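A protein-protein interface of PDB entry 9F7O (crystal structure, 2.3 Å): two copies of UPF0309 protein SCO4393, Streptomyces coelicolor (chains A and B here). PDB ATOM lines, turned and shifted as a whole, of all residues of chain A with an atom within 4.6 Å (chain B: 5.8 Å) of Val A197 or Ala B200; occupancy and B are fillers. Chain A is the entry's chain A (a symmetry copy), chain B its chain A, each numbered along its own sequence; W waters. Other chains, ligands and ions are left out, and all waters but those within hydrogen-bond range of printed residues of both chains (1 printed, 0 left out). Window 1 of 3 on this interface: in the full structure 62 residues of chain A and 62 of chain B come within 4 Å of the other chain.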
ATOM      1  N   ALA A  14     -24.764   8.583   6.624  1.00  0.00           N
ATOM      2  CA  ALA A  14     -23.751   9.166   7.497  1.00  0.00           C
ATOM      3  C   ALA A  14     -22.815  10.073   6.717  1.00  0.00           C
ATOM      4  O   ALA A  14     -22.399  11.126   7.214  1.00  0.00           O
ATOM      5  CB  ALA A  14     -22.933   8.082   8.198  1.00  0.00           C
ATOM      6  N   LEU A  18     -22.076  14.064   7.438  1.00  0.00           N
ATOM      7  CA  LEU A  18     -20.748  14.650   7.608  1.00  0.00           C
ATOM      8  C   LEU A  18     -20.486  15.756   6.587  1.00  0.00           C
ATOM      9  O   LEU A  18     -19.737  16.702   6.873  1.00  0.00           O
ATOM     10  CB  LEU A  18     -19.656  13.582   7.509  1.00  0.00           C
ATOM     11  CG  LEU A  18     -19.687  12.486   8.588  1.00  0.00           C
ATOM     12  CD1 LEU A  18     -18.540  11.486   8.352  1.00  0.00           C
ATOM     13  CD2 LEU A  18     -19.604  13.038   9.983  1.00  0.00           C
ATOM     14  N   ALA A 194     -27.280   7.435  13.395  1.00  0.00           N
ATOM     15  CA  ALA A 194     -25.954   7.937  13.045  1.00  0.00           C
ATOM     16  C   ALA A 194     -25.456   9.030  13.996  1.00  0.00           C
ATOM     17  O   ALA A 194     -24.400   9.625  13.748  1.00  0.00           O
ATOM     18  CB  ALA A 194     -25.938   8.459  11.600  1.00  0.00           C
ATOM     19  N   SER A 195     -26.164   9.285  15.101  1.00  0.00           N
ATOM     20  CA  SER A 195     -25.833  10.480  15.877  1.00  0.00           C
ATOM     21  C   SER A 195     -24.466  10.379  16.524  1.00  0.00           C
ATOM     22  O   SER A 195     -23.809  11.402  16.723  1.00  0.00           O
ATOM     23  CB  SER A 195     -26.885  10.761  16.948  1.00  0.00           C
ATOM     24  OG  SER A 195     -27.133   9.622  17.749  1.00  0.00           O
ATOM     25  N   THR A 196     -24.005   9.174  16.868  1.00  0.00           N
ATOM     26  CA  THR A 196     -22.677   9.082  17.476  1.00  0.00           C
ATOM     27  C   THR A 196     -21.580   9.279  16.440  1.00  0.00           C
ATOM     28  O   THR A 196     -20.552   9.917  16.725  1.00  0.00           O
ATOM     29  CB  THR A 196     -22.474   7.738  18.170  1.00  0.00           C
ATOM     30  OG1 THR A 196     -23.348   7.642  19.294  1.00  0.00           O
ATOM     31  CG2 THR A 196     -21.014   7.598  18.640  1.00  0.00           C
ATOM     32  N   VAL A 197     -21.771   8.694  15.247  1.00  0.00           N
ATOM     33  CA  VAL A 197     -20.877   8.952  14.120  1.00  0.00           C
ATOM     34  C   VAL A 197     -20.671  10.447  13.953  1.00  0.00           C
ATOM     35  O   VAL A 197     -19.538  10.946  13.890  1.00  0.00           O
ATOM     36  CB  VAL A 197     -21.447   8.326  12.831  1.00  0.00           C
ATOM     37  CG1 VAL A 197     -20.540   8.603  11.672  1.00  0.00           C
ATOM     38  CG2 VAL A 197     -21.686   6.829  13.016  1.00  0.00           C
ATOM     39  N   VAL A 198     -21.778  11.189  13.880  1.00  0.00           N
ATOM     40  CA  VAL A 198     -21.701  12.611  13.568  1.00  0.00           C
ATOM     41  C   VAL A 198     -21.124  13.391  14.738  1.00  0.00           C
ATOM     42  O   VAL A 198     -20.288  14.274  14.540  1.00  0.00           O
ATOM     43  CB  VAL A 198     -23.085  13.144  13.163  1.00  0.00           C
ATOM     44  CG1 VAL A 198     -23.092  14.642  13.042  1.00  0.00           C
ATOM     45  CG2 VAL A 198     -23.547  12.473  11.879  1.00  0.00           C
ATOM     46  N   THR A 199     -21.564  13.099  15.977  1.00  0.00           N
ATOM     47  CA  THR A 199     -21.048  13.889  17.088  1.00  0.00           C
ATOM     48  C   THR A 199     -19.576  13.587  17.358  1.00  0.00           C
ATOM     49  O   THR A 199     -18.840  14.480  17.773  1.00  0.00           O
ATOM     50  CB  THR A 199     -21.875  13.693  18.362  1.00  0.00           C
ATOM     51  OG1 THR A 199     -21.993  12.310  18.682  1.00  0.00           O
ATOM     52  CG2 THR A 199     -23.265  14.255  18.197  1.00  0.00           C
ATOM     53  N   ALA A 200     -19.117  12.354  17.133  1.00  0.00           N
ATOM     54  CA  ALA A 200     -17.687  12.092  17.302  1.00  0.00           C
ATOM     55  C   ALA A 200     -16.861  12.854  16.280  1.00  0.00           C
ATOM     56  O   ALA A 200     -15.799  13.398  16.605  1.00  0.00           O
ATOM     57  CB  ALA A 200     -17.374  10.600  17.177  1.00  0.00           C
ATOM     58  N   ALA A 201     -17.314  12.863  15.030  1.00  0.00           N
ATOM     59  CA  ALA A 201     -16.596  13.587  13.995  1.00  0.00           C
ATOM     60  C   ALA A 201     -16.599  15.077  14.282  1.00  0.00           C
ATOM     61  O   ALA A 201     -15.581  15.755  14.122  1.00  0.00           O
ATOM     62  CB  ALA A 201     -17.223  13.306  12.633  1.00  0.00           C
ATOM     63  N   LEU B  18     -15.332   6.378   5.405  1.00  0.00           N
ATOM     64  CA  LEU B  18     -16.660   5.774   5.307  1.00  0.00           C
ATOM     65  C   LEU B  18     -16.952   5.285   3.890  1.00  0.00           C
ATOM     66  O   LEU B  18     -17.699   4.313   3.709  1.00  0.00           O
ATOM     67  CB  LEU B  18     -17.747   6.753   5.755  1.00  0.00           C
ATOM     68  CG  LEU B  18     -17.683   7.204   7.225  1.00  0.00           C
ATOM     69  CD1 LEU B  18     -18.829   8.188   7.520  1.00  0.00           C
ATOM     70  CD2 LEU B  18     -17.736   6.054   8.190  1.00  0.00           C
ATOM     71  N   ALA B  57     -17.917   2.268  20.208  1.00  0.00           N
ATOM     72  CA  ALA B  57     -18.740   1.696  19.149  1.00  0.00           C
ATOM     73  C   ALA B  57     -19.560   0.514  19.665  1.00  0.00           C
ATOM     74  O   ALA B  57     -20.699   0.298  19.226  1.00  0.00           O
ATOM     75  CB  ALA B  57     -17.852   1.324  17.954  1.00  0.00           C
ATOM     76  N   ASP B  60     -22.508   1.978  21.324  1.00  0.00           N
ATOM     77  CA  ASP B  60     -23.397   2.681  20.408  1.00  0.00           C
ATOM     78  C   ASP B  60     -24.473   1.778  19.834  1.00  0.00           C
ATOM     79  O   ASP B  60     -25.427   2.277  19.228  1.00  0.00           O
ATOM     80  CB  ASP B  60     -22.582   3.296  19.273  1.00  0.00           C
ATOM     81  CG  ASP B  60     -23.342   4.390  18.523  1.00  0.00           C
ATOM     82  OD1 ASP B  60     -23.991   5.238  19.172  1.00  0.00           O
ATOM     83  OD2 ASP B  60     -23.261   4.418  17.274  1.00  0.00           O
ATOM     84  N   VAL B  61     -24.340   0.462  19.982  1.00  0.00           N
ATOM     85  CA  VAL B  61     -25.375  -0.453  19.521  1.00  0.00           C
ATOM     86  C   VAL B  61     -26.092  -1.128  20.674  1.00  0.00           C
ATOM     87  O   VAL B  61     -26.812  -2.097  20.447  1.00  0.00           O
ATOM     88  CB  VAL B  61     -24.812  -1.505  18.555  1.00  0.00           C
ATOM     89  CG1 VAL B  61     -24.378  -0.833  17.269  1.00  0.00           C
ATOM     90  CG2 VAL B  61     -23.673  -2.263  19.219  1.00  0.00           C
ATOM     91  N   SER B 195     -11.033   6.958  14.319  1.00  0.00           N
ATOM     92  CA  SER B 195     -11.353   5.536  14.441  1.00  0.00           C
ATOM     93  C   SER B 195     -12.704   5.308  15.090  1.00  0.00           C
ATOM     94  O   SER B 195     -13.362   4.309  14.794  1.00  0.00           O
ATOM     95  CB  SER B 195     -10.278   4.785  15.223  1.00  0.00           C
ATOM     96  OG  SER B 195     -10.004   5.406  16.464  1.00  0.00           O
ATOM     97  N   THR B 196     -13.149   6.201  15.977  1.00  0.00           N
ATOM     98  CA  THR B 196     -14.462   5.984  16.587  1.00  0.00           C
ATOM     99  C   THR B 196     -15.584   6.298  15.609  1.00  0.00           C
ATOM    100  O   THR B 196     -16.610   5.595  15.580  1.00  0.00           O
ATOM    101  CB  THR B 196     -14.640   6.835  17.842  1.00  0.00           C
ATOM    102  OG1 THR B 196     -13.739   6.390  18.854  1.00  0.00           O
ATOM    103  CG2 THR B 196     -16.088   6.725  18.356  1.00  0.00           C
ATOM    104  N   VAL B 197     -15.418   7.381  14.834  1.00  0.00           N
ATOM    105  CA  VAL B 197     -16.341   7.685  13.741  1.00  0.00           C
ATOM    106  C   VAL B 197     -16.559   6.449  12.888  1.00  0.00           C
ATOM    107  O   VAL B 197     -17.697   6.033  12.622  1.00  0.00           O
ATOM    108  CB  VAL B 197     -15.797   8.853  12.893  1.00  0.00           C
ATOM    109  CG1 VAL B 197     -16.734   9.155  11.764  1.00  0.00           C
ATOM    110  CG2 VAL B 197     -15.544  10.083  13.762  1.00  0.00           C
ATOM    111  N   VAL B 198     -15.459   5.838  12.444  1.00  0.00           N
ATOM    112  CA  VAL B 198     -15.552   4.736  11.495  1.00  0.00           C
ATOM    113  C   VAL B 198     -16.105   3.489  12.166  1.00  0.00           C
ATOM    114  O   VAL B 198     -16.952   2.801  11.592  1.00  0.00           O
ATOM    115  CB  VAL B 198     -14.181   4.468  10.852  1.00  0.00           C
ATOM    116  CG1 VAL B 198     -14.187   3.208  10.033  1.00  0.00           C
ATOM    117  CG2 VAL B 198     -13.746   5.671  10.032  1.00  0.00           C
ATOM    118  N   THR B 199     -15.635   3.158  13.383  1.00  0.00           N
ATOM    119  CA  THR B 199     -16.128   1.932  13.997  1.00  0.00           C
ATOM    120  C   THR B 199     -17.591   2.060  14.413  1.00  0.00           C
ATOM    121  O   THR B 199     -18.323   1.072  14.371  1.00  0.00           O
ATOM    122  CB  THR B 199     -15.270   1.503  15.191  1.00  0.00           C
ATOM    123  OG1 THR B 199     -15.137   2.568  16.127  1.00  0.00           O
ATOM    124  CG2 THR B 199     -13.888   1.095  14.745  1.00  0.00           C
ATOM    125  N   ALA B 200     -18.049   3.249  14.813  1.00  0.00           N
ATOM    126  CA  ALA B 200     -19.473   3.390  15.120  1.00  0.00           C
ATOM    127  C   ALA B 200     -20.328   3.201  13.879  1.00  0.00           C
ATOM    128  O   ALA B 200     -21.385   2.562  13.931  1.00  0.00           O
ATOM    129  CB  ALA B 200     -19.779   4.759  15.728  1.00  0.00           C
ATOM    130  N   ALA B 201     -19.904   3.791  12.765  1.00  0.00           N
ATOM    131  CA  ALA B 201     -20.651   3.643  11.527  1.00  0.00           C
ATOM    132  C   ALA B 201     -20.650   2.196  11.070  1.00  0.00           C
ATOM    133  O   ALA B 201     -21.676   1.670  10.631  1.00  0.00           O
ATOM    134  CB  ALA B 201     -20.054   4.542  10.449  1.00  0.00           C
ATOM    135  N   LEU B 202     -19.503   1.537  11.165  1.00  0.00           N
ATOM    136  CA  LEU B 202     -19.439   0.137  10.786  1.00  0.00           C
ATOM    137  C   LEU B 202     -20.364  -0.701  11.649  1.00  0.00           C
ATOM    138  O   LEU B 202     -21.103  -1.544  11.131  1.00  0.00           O
ATOM    139  CB  LEU B 202     -18.007  -0.346  10.896  1.00  0.00           C
ATOM    140  CG  LEU B 202     -17.548  -1.624  10.228  1.00  0.00           C
ATOM    141  CD1 LEU B 202     -18.166  -1.862   8.923  1.00  0.00           C
ATOM    142  CD2 LEU B 202     -16.013  -1.422  10.047  1.00  0.00           C
ATOM    143  N   MET B 203     -20.381  -0.449  12.967  1.00  0.00           N
ATOM    144  CA  MET B 203     -21.260  -1.239  13.830  1.00  0.00           C
ATOM    145  C   MET B 203     -22.738  -0.985  13.522  1.00  0.00           C
ATOM    146  O   MET B 203     -23.553  -1.922  13.560  1.00  0.00           O
ATOM    147  CB  MET B 203     -20.978  -0.952  15.304  1.00  0.00           C
ATOM    148  CG  MET B 203     -19.699  -1.576  15.829  1.00  0.00           C
ATOM    149  SD  MET B 203     -19.738  -3.407  15.833  1.00  0.00           S
ATOM    150  CE  MET B 203     -21.139  -3.662  16.948  1.00  0.00           C
ATOM    151  N   GLN B 204     -23.117   0.271  13.238  1.00  0.00           N
ATOM    152  CA  GLN B 204     -24.527   0.530  12.937  1.00  0.00           C
ATOM    153  C   GLN B 204     -24.955  -0.174  11.644  1.00  0.00           C
ATOM    154  O   GLN B 204     -26.086  -0.657  11.540  1.00  0.00           O
ATOM    155  CB  GLN B 204     -24.808   2.033  12.834  1.00  0.00           C
ATOM    156  CG  GLN B 204     -24.680   2.803  14.118  1.00  0.00           C
ATOM    157  CD  GLN B 204     -25.627   2.327  15.208  1.00  0.00           C
ATOM    158  OE1 GLN B 204     -26.674   1.731  14.956  1.00  0.00           O
ATOM    159  NE2 GLN B 204     -25.246   2.586  16.434  1.00  0.00           N
ATOM    160  N   ALA B 205     -24.068  -0.230  10.649  1.00  0.00           N
ATOM    161  CA  ALA B 205     -24.363  -0.946   9.410  1.00  0.00           C
ATOM    162  C   ALA B 205     -24.593  -2.425   9.676  1.00  0.00           C
ATOM    163  O   ALA B 205     -25.546  -3.028   9.169  1.00  0.00           O
ATOM    164  CB  ALA B 205     -23.206  -0.758   8.432  1.00  0.00           C
HETATM  165  O   HOH W   1     -24.460   6.460  15.840  1.00  0.00           O
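O of Asp B60 sits at hydrogen-bond distance from NE2 of Gln B204 (2.8 Å). The side-chain hydroxyl (OG1) of Thr A199 lies within hydrogen-bond range of the backbone carbonyl oxygen (O) of Thr A196 (3.4 Å).
The side-chain hydroxyl (OG1) of Thr A196 is in hydrogen-bond range of the side-chain carboxylate (OD1) of Asp B60, at 2.5 Å.
Of the 10 printed residues of chain A, 5 touch a printed residue of chain B. Among the printed residues, no Asp or Glu carboxylate lies within 4 Å of a Lys or Arg side-chain nitrogen of the other chain.
Water W1 lies within hydrogen-bond range of the side-chain carboxylate of Asp B60, the backbone NH of Thr A196 and the backbone NH of Ser A195.
Of the printed residues of chain B, Leu A18 touches Leu B18 (3.4 Å). Of the printed residues of chain B, Thr A196 touches Asp B60. Of chain B, only Val B197 (3.8 Å), Ala B200 (3.9 Å) and Ala B201 (3.5 Å) come within 4 Å of Val A197. Printed residues of chain B within 4 Å of Ala A201: Val B197 (3.5 Å). Of chain A, only Val A197 (3.9 Å) comes within 4 Å of Ala B200. Leu B202 touches none of the printed residues of chain A. The nearest residue of chain B that does not touch Val A197 is Leu B18 (4.5 Å).
Leu A18 touches Leu B18. Val A197 touches Val B197. CB of Ala B200 touches CG2 of Val A197, at 3.9 Å. Val A197 touches Ala B201 (CG2 to N, 3.5 Å). Val B197 touches Ala A200. Ala A201 touches Val B197.
Leu A18 touches its own counterpart, Leu B18. Val A197 touches its own counterpart, Val B197. Val A197 touches Ala B200, and with the chains exchanged Ala A200 touches Val B197. Val A197 touches Ala B201, and with the chains exchanged Ala A201 touches Val B197.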
